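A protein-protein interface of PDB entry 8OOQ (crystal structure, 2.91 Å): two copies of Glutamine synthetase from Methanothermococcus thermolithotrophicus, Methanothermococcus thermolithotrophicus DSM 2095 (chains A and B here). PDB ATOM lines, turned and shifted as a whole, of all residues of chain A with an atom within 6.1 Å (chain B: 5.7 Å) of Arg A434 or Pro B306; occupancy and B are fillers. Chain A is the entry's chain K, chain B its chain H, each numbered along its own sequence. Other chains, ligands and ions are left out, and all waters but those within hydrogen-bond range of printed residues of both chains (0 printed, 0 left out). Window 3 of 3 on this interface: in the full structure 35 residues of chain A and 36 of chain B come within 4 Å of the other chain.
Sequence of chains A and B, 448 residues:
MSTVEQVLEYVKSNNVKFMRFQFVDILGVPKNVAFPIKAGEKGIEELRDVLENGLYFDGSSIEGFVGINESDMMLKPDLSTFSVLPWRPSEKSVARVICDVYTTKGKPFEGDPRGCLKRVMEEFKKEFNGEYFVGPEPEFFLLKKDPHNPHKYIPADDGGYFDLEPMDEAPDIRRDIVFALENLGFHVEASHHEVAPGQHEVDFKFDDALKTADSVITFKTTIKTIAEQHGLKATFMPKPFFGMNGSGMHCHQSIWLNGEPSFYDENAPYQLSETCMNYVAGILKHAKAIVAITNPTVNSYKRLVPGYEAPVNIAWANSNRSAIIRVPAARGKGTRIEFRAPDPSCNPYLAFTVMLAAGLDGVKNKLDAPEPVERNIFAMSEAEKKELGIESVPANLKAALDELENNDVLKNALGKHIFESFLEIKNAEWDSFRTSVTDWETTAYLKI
O of Phe A433 touches NZ of Lys B302 (3.8 Å). O of Arg A434 touches CE of Lys B302, 3.1 Å away. Arg A434 touches Val B305 (NH1 to CG2, 3.3 Å). Arg A434 touches Tyr B308. Thr A435 touches Lys B302. CG2 of Val B305 touches CG2 of Thr A435, at 3.9 Å. CG2 of Thr A435 touches CE1 of Tyr B308 (3.8 Å).
O of Ser A432 is in hydrogen-bond range of OG1 of Thr A435. O of Asp A431 lies within hydrogen-bond range of OG1 of Thr A435 (2.8 Å). The guanidinium group (NH2) of Arg A434 is in salt-bridge range of the side-chain carboxylate (OD2) of Asp A431 (3.4 Å). O of Phe A433 lies within hydrogen-bond range of OG of Ser A436 (3.0 Å).
Of the 9 printed residues of chain A, 5 touch a printed residue of chain B. Among the printed residues, no Asp or Glu carboxylate lies within 4 Å of a Lys or Arg side-chain nitrogen of the other chain.
Trp A430 touches none of the printed residues of chain B. Arg A434 touches four residues of chain B. Of the printed residues of chain B, Ser A436 touches Lys B302. Printed residues of chain A within 4 Å of Val B305: Arg A434 (3.3 Å) and Thr A435 (3.9 Å). Pro B306 touches just one residue of chain A: Arg A434 (2.8 Å). Ser B392 touches none of the printed residues of chain A. The nearest residue of chain B that does not touch Arg A434 is Tyr B301 (4.2 Å). The nearest residue of chain A that does not touch Pro B306 is Asp A431 (5.7 Å).
The guanidinium group (NH2) of Arg A434 sits at hydrogen-bond distance from the backbone carbonyl oxygen (O) of Pro B306, 2.8 Å away. OD2 of Asp A431 is in hydrogen-bond range of OH of Tyr B308, 3.1 Å away. The side-chain amino group (NZ) of Lys B302 is in hydrogen-bond range of the backbone carbonyl oxygen (O) of Ser A436 (2.9 Å).
No position is printed for both chains.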
ATOM      1  N   ASN A 427     -13.679   7.425  15.910  1.00  0.00           N
ATOM      2  CA  ASN A 427     -13.937   7.054  14.512  1.00  0.00           C
ATOM      3  C   ASN A 427     -15.108   6.075  14.447  1.00  0.00           C
ATOM      4  O   ASN A 427     -15.918   6.174  13.532  1.00  0.00           O
ATOM      5  CB  ASN A 427     -12.704   6.446  13.827  1.00  0.00           C
ATOM      6  CG  ASN A 427     -11.783   7.467  13.194  1.00  0.00           C
ATOM      7  OD1 ASN A 427     -12.196   8.252  12.335  1.00  0.00           O
ATOM      8  ND2 ASN A 427     -10.516   7.485  13.589  1.00  0.00           N
ATOM      9  N   GLU A 429     -17.553   6.049  16.620  1.00  0.00           N
ATOM     10  CA  GLU A 429     -18.664   6.930  16.985  1.00  0.00           C
ATOM     11  C   GLU A 429     -19.108   7.732  15.758  1.00  0.00           C
ATOM     12  O   GLU A 429     -20.305   7.901  15.540  1.00  0.00           O
ATOM     13  CB  GLU A 429     -18.224   7.879  18.114  1.00  0.00           C
ATOM     14  CG  GLU A 429     -19.329   8.725  18.715  1.00  0.00           C
ATOM     15  CD  GLU A 429     -18.868   9.532  19.913  1.00  0.00           C
ATOM     16  OE1 GLU A 429     -18.162   8.964  20.777  1.00  0.00           O
ATOM     17  OE2 GLU A 429     -19.202  10.735  19.988  1.00  0.00           O
ATOM     18  N   TRP A 430     -18.145   8.228  14.964  1.00  0.00           N
ATOM     19  CA  TRP A 430     -18.427   8.976  13.742  1.00  0.00           C
ATOM     20  C   TRP A 430     -19.057   8.062  12.689  1.00  0.00           C
ATOM     21  O   TRP A 430     -20.002   8.474  12.018  1.00  0.00           O
ATOM     22  CB  TRP A 430     -17.138   9.608  13.181  1.00  0.00           C
ATOM     23  CG  TRP A 430     -17.336  10.300  11.866  1.00  0.00           C
ATOM     24  CD1 TRP A 430     -16.980   9.837  10.635  1.00  0.00           C
ATOM     25  CD2 TRP A 430     -18.070  11.508  11.645  1.00  0.00           C
ATOM     26  NE1 TRP A 430     -17.385  10.722   9.664  1.00  0.00           N
ATOM     27  CE2 TRP A 430     -18.092  11.737  10.255  1.00  0.00           C
ATOM     28  CE3 TRP A 430     -18.704  12.424  12.488  1.00  0.00           C
ATOM     29  CZ2 TRP A 430     -18.672  12.875   9.699  1.00  0.00           C
ATOM     30  CZ3 TRP A 430     -19.300  13.536  11.932  1.00  0.00           C
ATOM     31  CH2 TRP A 430     -19.282  13.753  10.555  1.00  0.00           C
ATOM     32  N   ASP A 431     -18.532   6.833  12.535  1.00  0.00           N
ATOM     33  CA  ASP A 431     -19.070   5.870  11.574  1.00  0.00           C
ATOM     34  C   ASP A 431     -20.515   5.517  11.904  1.00  0.00           C
ATOM     35  O   ASP A 431     -21.314   5.346  10.989  1.00  0.00           O
ATOM     36  CB  ASP A 431     -18.216   4.592  11.502  1.00  0.00           C
ATOM     37  CG  ASP A 431     -17.002   4.711  10.604  1.00  0.00           C
ATOM     38  OD1 ASP A 431     -16.317   5.756  10.667  1.00  0.00           O
ATOM     39  OD2 ASP A 431     -16.740   3.762   9.833  1.00  0.00           O
ATOM     40  N   SER A 432     -20.859   5.424  13.196  1.00  0.00           N
ATOM     41  CA  SER A 432     -22.229   5.143  13.617  1.00  0.00           C
ATOM     42  C   SER A 432     -23.167   6.285  13.211  1.00  0.00           C
ATOM     43  O   SER A 432     -24.311   6.028  12.846  1.00  0.00           O
ATOM     44  CB  SER A 432     -22.291   4.945  15.127  1.00  0.00           C
ATOM     45  OG  SER A 432     -23.621   4.707  15.555  1.00  0.00           O
ATOM     46  N   PHE A 433     -22.683   7.539  13.271  1.00  0.00           N
ATOM     47  CA  PHE A 433     -23.459   8.720  12.905  1.00  0.00           C
ATOM     48  C   PHE A 433     -23.681   8.821  11.388  1.00  0.00           C
ATOM     49  O   PHE A 433     -24.811   9.046  10.960  1.00  0.00           O
ATOM     50  CB  PHE A 433     -22.774   9.998  13.438  1.00  0.00           C
ATOM     51  CG  PHE A 433     -23.359  11.288  12.911  1.00  0.00           C
ATOM     52  CD1 PHE A 433     -24.627  11.693  13.281  1.00  0.00           C
ATOM     53  CD2 PHE A 433     -22.659  12.068  12.008  1.00  0.00           C
ATOM     54  CE1 PHE A 433     -25.169  12.870  12.788  1.00  0.00           C
ATOM     55  CE2 PHE A 433     -23.206  13.242  11.511  1.00  0.00           C
ATOM     56  CZ  PHE A 433     -24.455  13.638  11.908  1.00  0.00           C
ATOM     57  N   ARG A 434     -22.618   8.683  10.581  1.00  0.00           N
ATOM     58  CA  ARG A 434     -22.733   8.814   9.128  1.00  0.00           C
ATOM     59  C   ARG A 434     -23.536   7.692   8.453  1.00  0.00           C
ATOM     60  O   ARG A 434     -23.993   7.884   7.332  1.00  0.00           O
ATOM     61  CB  ARG A 434     -21.344   8.953   8.481  1.00  0.00           C
ATOM     62  CG  ARG A 434     -20.567   7.652   8.375  1.00  0.00           C
ATOM     63  CD  ARG A 434     -19.077   7.916   8.332  1.00  0.00           C
ATOM     64  NE  ARG A 434     -18.290   6.706   8.089  1.00  0.00           N
ATOM     65  CZ  ARG A 434     -18.135   6.120   6.906  1.00  0.00           C
ATOM     66  NH1 ARG A 434     -18.734   6.614   5.827  1.00  0.00           N
ATOM     67  NH2 ARG A 434     -17.389   5.027   6.790  1.00  0.00           N
ATOM     68  N   THR A 435     -23.686   6.526   9.103  1.00  0.00           N
ATOM     69  CA  THR A 435     -24.455   5.411   8.545  1.00  0.00           C
ATOM     70  C   THR A 435     -25.927   5.463   8.967  1.00  0.00           C
ATOM     71  O   THR A 435     -26.776   4.963   8.233  1.00  0.00           O
ATOM     72  CB  THR A 435     -23.853   4.067   8.977  1.00  0.00           C
ATOM     73  OG1 THR A 435     -23.713   4.042  10.402  1.00  0.00           O
ATOM     74  CG2 THR A 435     -22.526   3.762   8.284  1.00  0.00           C
ATOM     75  N   SER A 436     -26.237   6.040  10.142  1.00  0.00           N
ATOM     76  CA  SER A 436     -27.610   6.108  10.643  1.00  0.00           C
ATOM     77  C   SER A 436     -28.487   7.053   9.833  1.00  0.00           C
ATOM     78  O   SER A 436     -28.033   8.129   9.444  1.00  0.00           O
ATOM     79  CB  SER A 436     -27.625   6.545  12.107  1.00  0.00           C
ATOM     80  OG  SER A 436     -27.272   7.910  12.271  1.00  0.00           O
ATOM     81  N   TYR B 301     -25.690   9.351   0.714  1.00  0.00           N
ATOM     82  CA  TYR B 301     -24.408   8.908   1.261  1.00  0.00           C
ATOM     83  C   TYR B 301     -24.539   8.015   2.517  1.00  0.00           C
ATOM     84  O   TYR B 301     -23.531   7.710   3.151  1.00  0.00           O
ATOM     85  CB  TYR B 301     -23.496  10.120   1.497  1.00  0.00           C
ATOM     86  CG  TYR B 301     -23.261  10.856   0.198  1.00  0.00           C
ATOM     87  CD1 TYR B 301     -24.154  11.823  -0.239  1.00  0.00           C
ATOM     88  CD2 TYR B 301     -22.290  10.429  -0.696  1.00  0.00           C
ATOM     89  CE1 TYR B 301     -24.033  12.406  -1.492  1.00  0.00           C
ATOM     90  CE2 TYR B 301     -22.147  11.016  -1.945  1.00  0.00           C
ATOM     91  CZ  TYR B 301     -23.013  12.016  -2.334  1.00  0.00           C
ATOM     92  OH  TYR B 301     -22.887  12.584  -3.578  1.00  0.00           O
ATOM     93  N   LYS B 302     -25.766   7.552   2.829  1.00  0.00           N
ATOM     94  CA  LYS B 302     -26.051   6.553   3.860  1.00  0.00           C
ATOM     95  C   LYS B 302     -26.225   5.172   3.154  1.00  0.00           C
ATOM     96  O   LYS B 302     -25.945   4.150   3.773  1.00  0.00           O
ATOM     97  CB  LYS B 302     -27.287   6.928   4.712  1.00  0.00           C
ATOM     98  CG  LYS B 302     -26.986   7.840   5.912  1.00  0.00           C
ATOM     99  CD  LYS B 302     -26.723   9.291   5.516  1.00  0.00           C
ATOM    100  CE  LYS B 302     -25.988  10.093   6.567  1.00  0.00           C
ATOM    101  NZ  LYS B 302     -26.700  10.130   7.872  1.00  0.00           N
ATOM    102  N   LEU B 304     -24.881   4.841  -0.341  1.00  0.00           N
ATOM    103  CA  LEU B 304     -23.571   4.912  -0.996  1.00  0.00           C
ATOM    104  C   LEU B 304     -22.553   5.381   0.051  1.00  0.00           C
ATOM    105  O   LEU B 304     -21.979   6.465  -0.068  1.00  0.00           O
ATOM    106  CB  LEU B 304     -23.666   5.912  -2.168  1.00  0.00           C
ATOM    107  CG  LEU B 304     -22.470   6.025  -3.099  1.00  0.00           C
ATOM    108  CD1 LEU B 304     -22.497   4.939  -4.139  1.00  0.00           C
ATOM    109  CD2 LEU B 304     -22.445   7.378  -3.775  1.00  0.00           C
ATOM    110  N   VAL B 305     -22.336   4.550   1.076  1.00  0.00           N
ATOM    111  CA  VAL B 305     -21.472   4.877   2.210  1.00  0.00           C
ATOM    112  C   VAL B 305     -20.072   4.224   2.112  1.00  0.00           C
ATOM    113  O   VAL B 305     -19.991   2.996   2.168  1.00  0.00           O
ATOM    114  CB  VAL B 305     -22.188   4.535   3.549  1.00  0.00           C
ATOM    115  CG1 VAL B 305     -22.656   3.079   3.602  1.00  0.00           C
ATOM    116  CG2 VAL B 305     -21.311   4.870   4.746  1.00  0.00           C
ATOM    117  N   PRO B 306     -18.953   4.995   2.007  1.00  0.00           N
ATOM    118  CA  PRO B 306     -17.627   4.345   1.955  1.00  0.00           C
ATOM    119  C   PRO B 306     -17.293   3.540   3.208  1.00  0.00           C
ATOM    120  O   PRO B 306     -17.834   3.806   4.278  1.00  0.00           O
ATOM    121  CB  PRO B 306     -16.647   5.512   1.773  1.00  0.00           C
ATOM    122  CG  PRO B 306     -17.455   6.646   1.331  1.00  0.00           C
ATOM    123  CD  PRO B 306     -18.827   6.463   1.906  1.00  0.00           C
ATOM    124  N   GLY B 307     -16.420   2.548   3.059  1.00  0.00           N
ATOM    125  CA  GLY B 307     -16.041   1.672   4.163  1.00  0.00           C
ATOM    126  C   GLY B 307     -17.048   0.572   4.465  1.00  0.00           C
ATOM    127  O   GLY B 307     -16.759  -0.305   5.282  1.00  0.00           O
ATOM    128  N   TYR B 308     -18.247   0.612   3.835  1.00  0.00           N
ATOM    129  CA  TYR B 308     -19.309  -0.382   4.021  1.00  0.00           C
ATOM    130  C   TYR B 308     -19.811  -0.901   2.666  1.00  0.00           C
ATOM    131  O   TYR B 308     -19.601  -0.253   1.639  1.00  0.00           O
ATOM    132  CB  TYR B 308     -20.465   0.222   4.834  1.00  0.00           C
ATOM    133  CG  TYR B 308     -20.069   0.591   6.247  1.00  0.00           C
ATOM    134  CD1 TYR B 308     -19.501   1.824   6.532  1.00  0.00           C
ATOM    135  CD2 TYR B 308     -20.266  -0.292   7.298  1.00  0.00           C
ATOM    136  CE1 TYR B 308     -19.105   2.156   7.822  1.00  0.00           C
ATOM    137  CE2 TYR B 308     -19.896   0.038   8.596  1.00  0.00           C
ATOM    138  CZ  TYR B 308     -19.321   1.267   8.856  1.00  0.00           C
ATOM    139  OH  TYR B 308     -18.944   1.610  10.134  1.00  0.00           O
ATOM    140  N   VAL B 312     -19.246   1.850  -3.989  1.00  0.00           N
ATOM    141  CA  VAL B 312     -18.374   2.976  -3.629  1.00  0.00           C
ATOM    142  C   VAL B 312     -16.968   2.854  -4.213  1.00  0.00           C
ATOM    143  O   VAL B 312     -16.283   3.863  -4.352  1.00  0.00           O
ATOM    144  CB  VAL B 312     -18.276   3.121  -2.082  1.00  0.00           C
ATOM    145  CG1 VAL B 312     -19.593   3.607  -1.485  1.00  0.00           C
ATOM    146  CG2 VAL B 312     -17.826   1.815  -1.416  1.00  0.00           C
ATOM    147  N   SER B 392     -12.185   5.487  -3.361  1.00  0.00           N
ATOM    148  CA  SER B 392     -13.606   5.432  -3.002  1.00  0.00           C
ATOM    149  C   SER B 392     -14.324   6.755  -3.295  1.00  0.00           C
ATOM    150  O   SER B 392     -13.699   7.816  -3.284  1.00  0.00           O
ATOM    151  CB  SER B 392     -13.764   5.066  -1.530  1.00  0.00           C
ATOM    152  OG  SER B 392     -13.267   3.761  -1.275  1.00  0.00           O
ATOM    153  N   VAL B 393     -15.638   6.682  -3.566  1.00  0.00           N
ATOM    154  CA  VAL B 393     -16.459   7.867  -3.850  1.00  0.00           C
ATOM    155  C   VAL B 393     -16.648   8.697  -2.568  1.00  0.00           C
ATOM    156  O   VAL B 393     -16.663   8.123  -1.481  1.00  0.00           O
ATOM    157  CB  VAL B 393     -17.834   7.499  -4.476  1.00  0.00           C
ATOM    158  CG1 VAL B 393     -17.661   6.704  -5.764  1.00  0.00           C
ATOM    159  CG2 VAL B 393     -18.733   6.765  -3.482  1.00  0.00           C
ATOM    160  N   PRO B 394     -16.837  10.034  -2.660  1.00  0.00           N
ATOM    161  CA  PRO B 394     -16.993  10.844  -1.431  1.00  0.00           C
ATOM    162  C   PRO B 394     -17.958  10.298  -0.373  1.00  0.00           C
ATOM    163  O   PRO B 394     -18.961   9.669  -0.703  1.00  0.00           O
ATOM    164  CB  PRO B 394     -17.466  12.209  -1.950  1.00  0.00           C
ATOM    165  CG  PRO B 394     -17.514  12.111  -3.440  1.00  0.00           C
ATOM    166  CD  PRO B 394     -16.803  10.886  -3.865  1.00  0.00           C
ATOM    167  N   ALA B 395     -17.639  10.541   0.909  1.00  0.00           N
ATOM    168  CA  ALA B 395     -18.423  10.057   2.044  1.00  0.00           C
ATOM    169  C   ALA B 395     -19.674  10.880   2.359  1.00  0.00           C
ATOM    170  O   ALA B 395     -20.514  10.397   3.114  1.00  0.00           O
ATOM    171  CB  ALA B 395     -17.539   9.995   3.279  1.00  0.00           C
